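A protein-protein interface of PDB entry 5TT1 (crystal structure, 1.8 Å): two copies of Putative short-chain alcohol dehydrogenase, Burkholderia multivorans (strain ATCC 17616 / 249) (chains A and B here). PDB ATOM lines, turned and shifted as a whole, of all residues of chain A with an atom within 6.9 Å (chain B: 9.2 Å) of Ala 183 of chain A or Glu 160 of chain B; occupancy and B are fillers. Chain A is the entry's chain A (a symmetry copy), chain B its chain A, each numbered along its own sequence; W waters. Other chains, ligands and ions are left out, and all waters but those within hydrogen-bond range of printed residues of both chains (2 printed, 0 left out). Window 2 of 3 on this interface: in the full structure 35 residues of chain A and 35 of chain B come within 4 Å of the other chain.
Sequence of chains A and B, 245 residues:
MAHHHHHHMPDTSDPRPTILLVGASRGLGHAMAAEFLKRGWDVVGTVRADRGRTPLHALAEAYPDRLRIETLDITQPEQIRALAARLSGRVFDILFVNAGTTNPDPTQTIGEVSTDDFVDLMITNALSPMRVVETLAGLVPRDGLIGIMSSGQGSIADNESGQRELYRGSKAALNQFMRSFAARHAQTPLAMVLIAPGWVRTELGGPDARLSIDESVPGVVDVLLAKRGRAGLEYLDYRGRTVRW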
ATOM      1  N   MET A 178     -17.850 -10.069  -8.188  1.00  0.00           N
ATOM      2  CA  MET A 178     -17.082  -8.833  -8.227  1.00  0.00           C
ATOM      3  C   MET A 178     -15.867  -8.959  -9.140  1.00  0.00           C
ATOM      4  O   MET A 178     -15.518  -8.004  -9.838  1.00  0.00           O
ATOM      5  CB  MET A 178     -16.671  -8.432  -6.812  1.00  0.00           C
ATOM      6  CG  MET A 178     -16.156  -6.996  -6.727  1.00  0.00           C
ATOM      7  SD  MET A 178     -17.394  -5.809  -7.310  1.00  0.00           S
ATOM      8  CE  MET A 178     -16.361  -4.359  -7.541  1.00  0.00           C
ATOM      9  N   ARG A 179     -15.208 -10.127  -9.159  1.00  0.00           N
ATOM     10  CA  ARG A 179     -14.089 -10.297 -10.080  1.00  0.00           C
ATOM     11  C   ARG A 179     -14.535 -10.136 -11.529  1.00  0.00           C
ATOM     12  O   ARG A 179     -13.813  -9.552 -12.343  1.00  0.00           O
ATOM     13  CB  ARG A 179     -13.417 -11.659  -9.885  1.00  0.00           C
ATOM     14  CG  ARG A 179     -12.597 -11.794  -8.601  1.00  0.00           C
ATOM     15  CD  ARG A 179     -11.310 -12.569  -8.882  1.00  0.00           C
ATOM     16  NE  ARG A 179     -10.277 -11.736  -9.509  1.00  0.00           N
ATOM     17  CZ  ARG A 179      -9.182 -12.208 -10.096  1.00  0.00           C
ATOM     18  NH1 ARG A 179      -8.306 -11.368 -10.635  1.00  0.00           N
ATOM     19  NH2 ARG A 179      -8.962 -13.517 -10.166  1.00  0.00           N
ATOM     20  N   SER A 180     -15.726 -10.638 -11.876  1.00  0.00           N
ATOM     21  CA  SER A 180     -16.184 -10.457 -13.250  1.00  0.00           C
ATOM     22  C   SER A 180     -16.470  -8.991 -13.544  1.00  0.00           C
ATOM     23  O   SER A 180     -16.148  -8.495 -14.630  1.00  0.00           O
ATOM     24  CB  SER A 180     -17.425 -11.300 -13.524  1.00  0.00           C
ATOM     25  OG  SER A 180     -17.112 -12.679 -13.520  1.00  0.00           O
ATOM     26  N   PHE A 181     -17.112  -8.296 -12.599  1.00  0.00           N
ATOM     27  CA  PHE A 181     -17.304  -6.854 -12.730  1.00  0.00           C
ATOM     28  C   PHE A 181     -15.969  -6.149 -12.941  1.00  0.00           C
ATOM     29  O   PHE A 181     -15.853  -5.256 -13.791  1.00  0.00           O
ATOM     30  CB  PHE A 181     -18.034  -6.331 -11.482  1.00  0.00           C
ATOM     31  CG  PHE A 181     -18.250  -4.843 -11.464  1.00  0.00           C
ATOM     32  CD1 PHE A 181     -19.409  -4.291 -11.985  1.00  0.00           C
ATOM     33  CD2 PHE A 181     -17.307  -3.997 -10.898  1.00  0.00           C
ATOM     34  CE1 PHE A 181     -19.618  -2.915 -11.955  1.00  0.00           C
ATOM     35  CE2 PHE A 181     -17.505  -2.613 -10.874  1.00  0.00           C
ATOM     36  CZ  PHE A 181     -18.664  -2.079 -11.396  1.00  0.00           C
ATOM     37  N   ALA A 182     -14.941  -6.558 -12.196  1.00  0.00           N
ATOM     38  CA  ALA A 182     -13.618  -5.959 -12.374  1.00  0.00           C
ATOM     39  C   ALA A 182     -13.080  -6.198 -13.781  1.00  0.00           C
ATOM     40  O   ALA A 182     -12.477  -5.299 -14.397  1.00  0.00           O
ATOM     41  CB  ALA A 182     -12.654  -6.522 -11.328  1.00  0.00           C
ATOM     42  N   ALA A 183     -13.273  -7.410 -14.305  1.00  0.00           N
ATOM     43  CA  ALA A 183     -12.825  -7.710 -15.662  1.00  0.00           C
ATOM     44  C   ALA A 183     -13.422  -6.731 -16.666  1.00  0.00           C
ATOM     45  O   ALA A 183     -12.737  -6.285 -17.598  1.00  0.00           O
ATOM     46  CB  ALA A 183     -13.197  -9.147 -16.028  1.00  0.00           C
ATOM     47  N   ARG A 184     -14.694  -6.371 -16.481  1.00  0.00           N
ATOM     48  CA  ARG A 184     -15.345  -5.418 -17.373  1.00  0.00           C
ATOM     49  C   ARG A 184     -14.731  -4.031 -17.292  1.00  0.00           C
ATOM     50  O   ARG A 184     -14.935  -3.222 -18.203  1.00  0.00           O
ATOM     51  CB  ARG A 184     -16.843  -5.350 -17.060  1.00  0.00           C
ATOM     52  CG  ARG A 184     -17.627  -6.524 -17.636  1.00  0.00           C
ATOM     53  CD  ARG A 184     -19.133  -6.385 -17.433  1.00  0.00           C
ATOM     54  NE  ARG A 184     -19.604  -6.947 -16.164  1.00  0.00           N
ATOM     55  CZ  ARG A 184     -20.348  -6.288 -15.276  1.00  0.00           C
ATOM     56  NH1 ARG A 184     -20.697  -5.021 -15.499  1.00  0.00           N
ATOM     57  NH2 ARG A 184     -20.758  -6.899 -14.166  1.00  0.00           N
ATOM     58  N   HIS A 185     -13.994  -3.731 -16.224  1.00  0.00           N
ATOM     59  CA  HIS A 185     -13.364  -2.432 -16.039  1.00  0.00           C
ATOM     60  C   HIS A 185     -11.849  -2.510 -16.161  1.00  0.00           C
ATOM     61  O   HIS A 185     -11.147  -1.580 -15.752  1.00  0.00           O
ATOM     62  CB  HIS A 185     -13.771  -1.846 -14.686  1.00  0.00           C
ATOM     63  CG  HIS A 185     -15.203  -1.414 -14.627  1.00  0.00           C
ATOM     64  ND1 HIS A 185     -16.230  -2.270 -14.280  1.00  0.00           N
ATOM     65  CD2 HIS A 185     -15.781  -0.217 -14.881  1.00  0.00           C
ATOM     66  CE1 HIS A 185     -17.378  -1.619 -14.328  1.00  0.00           C
ATOM     67  NE2 HIS A 185     -17.134  -0.371 -14.685  1.00  0.00           N
ATOM     68  N   ALA A 186     -11.337  -3.599 -16.732  1.00  0.00           N
ATOM     69  CA  ALA A 186      -9.897  -3.828 -16.744  1.00  0.00           C
ATOM     70  C   ALA A 186      -9.152  -2.743 -17.511  1.00  0.00           C
ATOM     71  O   ALA A 186      -7.989  -2.460 -17.200  1.00  0.00           O
ATOM     72  CB  ALA A 186      -9.597  -5.204 -17.334  1.00  0.00           C
ATOM     73  N   GLN A 187      -9.788  -2.118 -18.498  1.00  0.00           N
ATOM     74  CA  GLN A 187      -9.127  -1.070 -19.267  1.00  0.00           C
ATOM     75  C   GLN A 187      -9.245   0.310 -18.621  1.00  0.00           C
ATOM     76  O   GLN A 187      -8.727   1.285 -19.172  1.00  0.00           O
ATOM     77  CB  GLN A 187      -9.683  -1.033 -20.694  1.00  0.00           C
ATOM     78  N   MET A 192     -11.090  -0.893  -7.015  1.00  0.00           N
ATOM     79  CA  MET A 192     -12.115  -1.725  -6.396  1.00  0.00           C
ATOM     80  C   MET A 192     -11.509  -2.573  -5.286  1.00  0.00           C
ATOM     81  O   MET A 192     -10.363  -3.015  -5.393  1.00  0.00           O
ATOM     82  CB  MET A 192     -12.780  -2.639  -7.426  1.00  0.00           C
ATOM     83  CG  MET A 192     -13.583  -1.913  -8.475  1.00  0.00           C
ATOM     84  SD  MET A 192     -13.789  -2.940  -9.930  1.00  0.00           S
ATOM     85  CE  MET A 192     -12.155  -2.813 -10.655  1.00  0.00           C
ATOM     86  N   LEU A 233      -9.156  -4.531  -8.995  1.00  0.00           N
ATOM     87  CA  LEU A 233      -9.795  -5.139  -7.837  1.00  0.00           C
ATOM     88  C   LEU A 233      -8.774  -5.904  -7.002  1.00  0.00           C
ATOM     89  O   LEU A 233      -7.978  -6.679  -7.543  1.00  0.00           O
ATOM     90  CB  LEU A 233     -10.912  -6.082  -8.281  1.00  0.00           C
ATOM     91  CG  LEU A 233     -11.506  -6.908  -7.140  1.00  0.00           C
ATOM     92  CD1 LEU A 233     -12.178  -5.985  -6.129  1.00  0.00           C
ATOM     93  CD2 LEU A 233     -12.465  -7.972  -7.659  1.00  0.00           C
ATOM     94  N   TRP A 245      -8.050 -15.822  -2.797  1.00  0.00           N
ATOM     95  CA  TRP A 245      -9.400 -15.997  -3.309  1.00  0.00           C
ATOM     96  C   TRP A 245     -10.004 -17.327  -2.854  1.00  0.00           C
ATOM     97  O   TRP A 245     -11.235 -17.436  -2.738  1.00  0.00           O
ATOM     98  CB  TRP A 245      -9.410 -15.927  -4.843  1.00  0.00           C
ATOM     99  CG  TRP A 245      -8.985 -14.603  -5.426  1.00  0.00           C
ATOM    100  CD1 TRP A 245      -7.816 -14.336  -6.068  1.00  0.00           C
ATOM    101  CD2 TRP A 245      -9.733 -13.375  -5.430  1.00  0.00           C
ATOM    102  NE1 TRP A 245      -7.784 -13.023  -6.475  1.00  0.00           N
ATOM    103  CE2 TRP A 245      -8.946 -12.409  -6.090  1.00  0.00           C
ATOM    104  CE3 TRP A 245     -10.980 -12.996  -4.930  1.00  0.00           C
ATOM    105  CZ2 TRP A 245      -9.368 -11.092  -6.271  1.00  0.00           C
ATOM    106  CZ3 TRP A 245     -11.404 -11.693  -5.123  1.00  0.00           C
ATOM    107  CH2 TRP A 245     -10.599 -10.755  -5.779  1.00  0.00           C
ATOM    108  OXT TRP A 245      -9.288 -18.309  -2.615  1.00  0.00           O
ATOM    109  N   GLY B 152     -13.930 -24.984 -14.764  1.00  0.00           N
ATOM    110  CA  GLY B 152     -12.853 -24.013 -14.687  1.00  0.00           C
ATOM    111  C   GLY B 152     -13.347 -22.604 -14.476  1.00  0.00           C
ATOM    112  O   GLY B 152     -12.601 -21.766 -13.957  1.00  0.00           O
ATOM    113  N   GLN B 153     -14.598 -22.323 -14.858  1.00  0.00           N
ATOM    114  CA  GLN B 153     -15.212 -21.015 -14.626  1.00  0.00           C
ATOM    115  C   GLN B 153     -15.478 -20.749 -13.148  1.00  0.00           C
ATOM    116  O   GLN B 153     -15.674 -19.596 -12.756  1.00  0.00           O
ATOM    117  CB  GLN B 153     -16.522 -20.928 -15.412  1.00  0.00           C
ATOM    118  CG  GLN B 153     -16.332 -21.189 -16.883  1.00  0.00           C
ATOM    119  CD  GLN B 153     -15.625 -20.027 -17.563  1.00  0.00           C
ATOM    120  OE1 GLN B 153     -16.150 -18.914 -17.607  1.00  0.00           O
ATOM    121  NE2 GLN B 153     -14.417 -20.267 -18.057  1.00  0.00           N
ATOM    122  N   SER B 155     -13.315 -21.226 -10.694  1.00  0.00           N
ATOM    123  CA  SER B 155     -12.107 -20.785 -10.007  1.00  0.00           C
ATOM    124  C   SER B 155     -12.135 -19.270  -9.843  1.00  0.00           C
ATOM    125  O   SER B 155     -12.281 -18.546 -10.829  1.00  0.00           O
ATOM    126  CB  SER B 155     -10.877 -21.210 -10.802  1.00  0.00           C
ATOM    127  OG  SER B 155      -9.728 -20.510 -10.367  1.00  0.00           O
ATOM    128  N   ILE B 156     -11.993 -18.789  -8.605  1.00  0.00           N
ATOM    129  CA  ILE B 156     -11.952 -17.346  -8.388  1.00  0.00           C
ATOM    130  C   ILE B 156     -10.567 -16.796  -8.717  1.00  0.00           C
ATOM    131  O   ILE B 156     -10.448 -15.752  -9.365  1.00  0.00           O
ATOM    132  CB  ILE B 156     -12.389 -16.999  -6.949  1.00  0.00           C
ATOM    133  CG1 ILE B 156     -13.775 -17.584  -6.660  1.00  0.00           C
ATOM    134  CG2 ILE B 156     -12.408 -15.489  -6.743  1.00  0.00           C
ATOM    135  CD1 ILE B 156     -14.437 -17.048  -5.384  1.00  0.00           C
ATOM    136  N   ALA B 157      -9.497 -17.497  -8.316  1.00  0.00           N
ATOM    137  CA  ALA B 157      -8.161 -17.033  -8.679  1.00  0.00           C
ATOM    138  C   ALA B 157      -8.011 -16.875 -10.194  1.00  0.00           C
ATOM    139  O   ALA B 157      -7.382 -15.922 -10.664  1.00  0.00           O
ATOM    140  CB  ALA B 157      -7.098 -17.983  -8.131  1.00  0.00           C
ATOM    141  N   ASP B 158      -8.605 -17.780 -10.974  1.00  0.00           N
ATOM    142  CA  ASP B 158      -8.404 -17.769 -12.423  1.00  0.00           C
ATOM    143  C   ASP B 158      -9.302 -16.777 -13.162  1.00  0.00           C
ATOM    144  O   ASP B 158      -9.149 -16.624 -14.379  1.00  0.00           O
ATOM    145  CB  ASP B 158      -8.643 -19.171 -13.003  1.00  0.00           C
ATOM    146  CG  ASP B 158      -7.532 -20.143 -12.669  1.00  0.00           C
ATOM    147  OD1 ASP B 158      -6.493 -19.710 -12.105  1.00  0.00           O
ATOM    148  OD2 ASP B 158      -7.699 -21.349 -12.978  1.00  0.00           O
ATOM    149  N   ASN B 159     -10.236 -16.112 -12.481  1.00  0.00           N
ATOM    150  CA  ASN B 159     -11.226 -15.274 -13.164  1.00  0.00           C
ATOM    151  C   ASN B 159     -10.614 -13.903 -13.449  1.00  0.00           C
ATOM    152  O   ASN B 159     -10.823 -12.920 -12.731  1.00  0.00           O
ATOM    153  CB  ASN B 159     -12.507 -15.154 -12.349  1.00  0.00           C
ATOM    154  CG  ASN B 159     -13.558 -14.303 -13.052  1.00  0.00           C
ATOM    155  OD1 ASN B 159     -13.372 -13.898 -14.204  1.00  0.00           O
ATOM    156  ND2 ASN B 159     -14.663 -14.035 -12.372  1.00  0.00           N
ATOM    157  N   GLU B 160      -9.859 -13.845 -14.546  1.00  0.00           N
ATOM    158  CA  GLU B 160      -9.287 -12.599 -15.041  1.00  0.00           C
ATOM    159  C   GLU B 160     -10.121 -11.946 -16.133  1.00  0.00           C
ATOM    160  O   GLU B 160      -9.938 -10.754 -16.397  1.00  0.00           O
ATOM    161  CB  GLU B 160      -7.877 -12.843 -15.586  1.00  0.00           C
ATOM    162  CG  GLU B 160      -6.918 -13.416 -14.573  1.00  0.00           C
ATOM    163  CD  GLU B 160      -6.651 -12.465 -13.428  1.00  0.00           C
ATOM    164  OE1 GLU B 160      -6.601 -11.239 -13.674  1.00  0.00           O
ATOM    165  OE2 GLU B 160      -6.489 -12.948 -12.284  1.00  0.00           O
ATOM    166  N   SER B 161     -11.027 -12.692 -16.767  1.00  0.00           N
ATOM    167  CA  SER B 161     -11.711 -12.234 -17.962  1.00  0.00           C
ATOM    168  C   SER B 161     -13.214 -12.074 -17.802  1.00  0.00           C
ATOM    169  O   SER B 161     -13.858 -11.544 -18.715  1.00  0.00           O
ATOM    170  CB  SER B 161     -11.446 -13.205 -19.123  1.00  0.00           C
ATOM    171  OG  SER B 161     -12.034 -14.467 -18.850  1.00  0.00           O
ATOM    172  N   GLY B 162     -13.799 -12.509 -16.686  1.00  0.00           N
ATOM    173  CA  GLY B 162     -15.246 -12.425 -16.568  1.00  0.00           C
ATOM    174  C   GLY B 162     -15.946 -13.261 -17.624  1.00  0.00           C
ATOM    175  O   GLY B 162     -15.465 -14.332 -18.009  1.00  0.00           O
ATOM    176  N   GLN B 163     -17.081 -12.733 -18.120  1.00  0.00           N
ATOM    177  CA  GLN B 163     -18.001 -13.426 -19.024  1.00  0.00           C
ATOM    178  C   GLN B 163     -18.693 -14.575 -18.300  1.00  0.00           C
ATOM    179  O   GLN B 163     -18.186 -15.059 -17.284  1.00  0.00           O
ATOM    180  CB  GLN B 163     -17.274 -13.924 -20.278  1.00  0.00           C
ATOM    181  CG  GLN B 163     -16.569 -12.804 -21.052  1.00  0.00           C
ATOM    182  CD  GLN B 163     -15.872 -13.290 -22.306  1.00  0.00           C
ATOM    183  OE1 GLN B 163     -15.640 -14.484 -22.482  1.00  0.00           O
ATOM    184  NE2 GLN B 163     -15.531 -12.359 -23.188  1.00  0.00           N
ATOM    185  N   GLU B 165     -21.216 -14.584 -16.366  1.00  0.00           N
ATOM    186  CA  GLU B 165     -21.065 -14.105 -14.994  1.00  0.00           C
ATOM    187  C   GLU B 165     -21.912 -14.894 -14.009  1.00  0.00           C
ATOM    188  O   GLU B 165     -21.442 -15.229 -12.913  1.00  0.00           O
ATOM    189  CB  GLU B 165     -21.388 -12.613 -14.914  1.00  0.00           C
ATOM    190  CG  GLU B 165     -20.399 -11.782 -15.703  1.00  0.00           C
ATOM    191  CD  GLU B 165     -20.345 -10.342 -15.247  1.00  0.00           C
ATOM    192  OE1 GLU B 165     -21.099  -9.976 -14.314  1.00  0.00           O
ATOM    193  OE2 GLU B 165     -19.540  -9.579 -15.822  1.00  0.00           O
ATOM    194  N   ARG B 168     -20.428 -18.420 -13.510  1.00  0.00           N
ATOM    195  CA  ARG B 168     -19.214 -18.411 -12.698  1.00  0.00           C
ATOM    196  C   ARG B 168     -19.534 -18.343 -11.211  1.00  0.00           C
ATOM    197  O   ARG B 168     -18.932 -19.062 -10.400  1.00  0.00           O
ATOM    198  CB  ARG B 168     -18.325 -17.235 -13.090  1.00  0.00           C
ATOM    199  CG  ARG B 168     -17.632 -17.321 -14.422  1.00  0.00           C
ATOM    200  CD  ARG B 168     -16.726 -16.068 -14.498  1.00  0.00           C
ATOM    201  NE  ARG B 168     -15.757 -16.017 -15.586  1.00  0.00           N
ATOM    202  CZ  ARG B 168     -14.602 -16.681 -15.602  1.00  0.00           C
ATOM    203  NH1 ARG B 168     -14.277 -17.483 -14.594  1.00  0.00           N
ATOM    204  NH2 ARG B 168     -13.765 -16.535 -16.628  1.00  0.00           N
ATOM    205  N   ARG B 244      -6.612 -23.778  -9.413  1.00  0.00           N
ATOM    206  CA  ARG B 244      -6.619 -22.856  -8.289  1.00  0.00           C
ATOM    207  C   ARG B 244      -8.056 -22.564  -7.882  1.00  0.00           C
ATOM    208  O   ARG B 244      -8.954 -22.493  -8.725  1.00  0.00           O
ATOM    209  CB  ARG B 244      -5.876 -21.571  -8.645  1.00  0.00           C
ATOM    210  CG  ARG B 244      -4.373 -21.776  -8.832  1.00  0.00           C
ATOM    211  CD  ARG B 244      -3.642 -20.448  -8.963  1.00  0.00           C
ATOM    212  NE  ARG B 244      -4.214 -19.651 -10.038  1.00  0.00           N
ATOM    213  CZ  ARG B 244      -4.029 -18.348 -10.191  1.00  0.00           C
ATOM    214  NH1 ARG B 244      -3.269 -17.671  -9.337  1.00  0.00           N
ATOM    215  NH2 ARG B 244      -4.611 -17.722 -11.203  1.00  0.00           N
HETATM  216  O   HOH W   1     -19.257 -13.476 -12.315  1.00  0.00           O
HETATM  217  O   HOH W   2     -11.224 -10.120 -12.810  1.00  0.00           O
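Among the printed residues, pairs that only touch across the chains: Ser 180 of chain A with Gly 162 of chain B, Ser 180 of chain A with Glu 165 of chain B, Ser 180 of chain A with Arg 168 of chain B, Ala 183 of chain A with Glu 160 of chain B, Ala 183 of chain A with Ser 161 of chain B, Ala 183 of chain A with Gly 162 of chain B, Trp 245 of chain A with Ile 156 of chain B and Trp 245 of chain A with Ala 157 of chain B.
No position is printed for both chains.
N of Gly 162 of chain B is in hydrogen-bond range of OD1 of Asn 159 of chain B (2.9 Å). O of Gln 163 of chain B lies within hydrogen-bond range of NE of Arg 168 of chain B, 3.1 Å away. The guanidinium group (NH1) of Arg 168 of chain B is in hydrogen-bond range of the backbone carbonyl oxygen (O) of Gln 153 of chain B (3.1 Å). The guanidinium group of Arg 244 of chain B lies within hydrogen-bond range of the backbone carbonyl oxygen of Ala 157 of chain B, 3.3 Å away. The side-chain amide oxygen (OD1) of Asn 159 of chain B sits close to the guanidinium group (NE) of Arg 168 of chain B. The side-chain hydroxyl of Ser 161 of chain B sits at hydrogen-bond distance from the guanidinium group of Arg 168 of chain B, 3.5 Å away.
Ala 182 of chain A touches none of the printed residues of chain B. Of chain B, only Glu 160 (3.7 Å), Ser 161 (3.4 Å) and Gly 162 (3.5 Å) come within 4 Å of Ala 183 of chain A. Of the printed residues of chain B, Arg 184 of chain A touches Glu 165 (2.7 Å). Of the printed residues of chain A, Ile 156 of chain B touches Arg 179 and Trp 245. Glu 160 of chain B touches just these residues of chain A: Arg 179 (2.9 Å) and Ala 183 (3.7 Å). The nearest residue of chain A that does not touch Glu 160 of chain B is Ala 186 of chain A (5.6 Å).
Of the 13 printed residues of chain A, 5 touch a printed residue of chain B. Hydrophobic or aromatic side chains of chain A that line the printed part of chain B: Ala 183 and Trp 245. Of the 14 printed residues of chain B, 8 touch a printed residue of chain A. Printed residues of chain B that touch a printed residue of chain A: Ile 156, Ala 157, Asn 159, Glu 160, Ser 161, Gly 162, Glu 165 and Arg 168. Among the printed residues, Asp or Glu carboxylates within 4 Å of a Lys or Arg side-chain nitrogen of the other chain: Arg 179 of chain A with Glu 160 of chain B (2.9 Å) and Arg 184 of chain A with Glu 165 of chain B (2.7 Å).
Water W1 bridges OG of Ser 180 of chain A (2.6 Å) and O of Glu 165 of chain B (2.9 Å). Water W2 bridges the backbone carbonyl oxygen of Arg 179 of chain A (2.7 Å) and the backbone carbonyl oxygen of Asn 159 of chain B (2.8 Å).
The guanidinium group (NH2) of Arg 179 of chain A lies within hydrogen-bond range of the backbone carbonyl oxygen (O) of Ile 156 of chain B. NH2 of Arg 179 of chain A lies within hydrogen-bond range of O of Ala 157 of chain B (2.9 Å). NE of Arg 184 of chain A is in salt-bridge range of OE2 of Glu 165 of chain B, at 2.7 Å. The side-chain amide nitrogen (ND2) of Asn 159 of chain B lies within hydrogen-bond range of the side-chain hydroxyl (OG) of Ser 180 of chain A (3.0 Å). O of Asn 159 of chain B sits close to NH2 of Arg 179 of chain A. The guanidinium group (NH1) of Arg 179 of chain A is in salt-bridge range of the side-chain carboxylate (OE2) of Glu 160 of chain B, 2.9 Å away.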
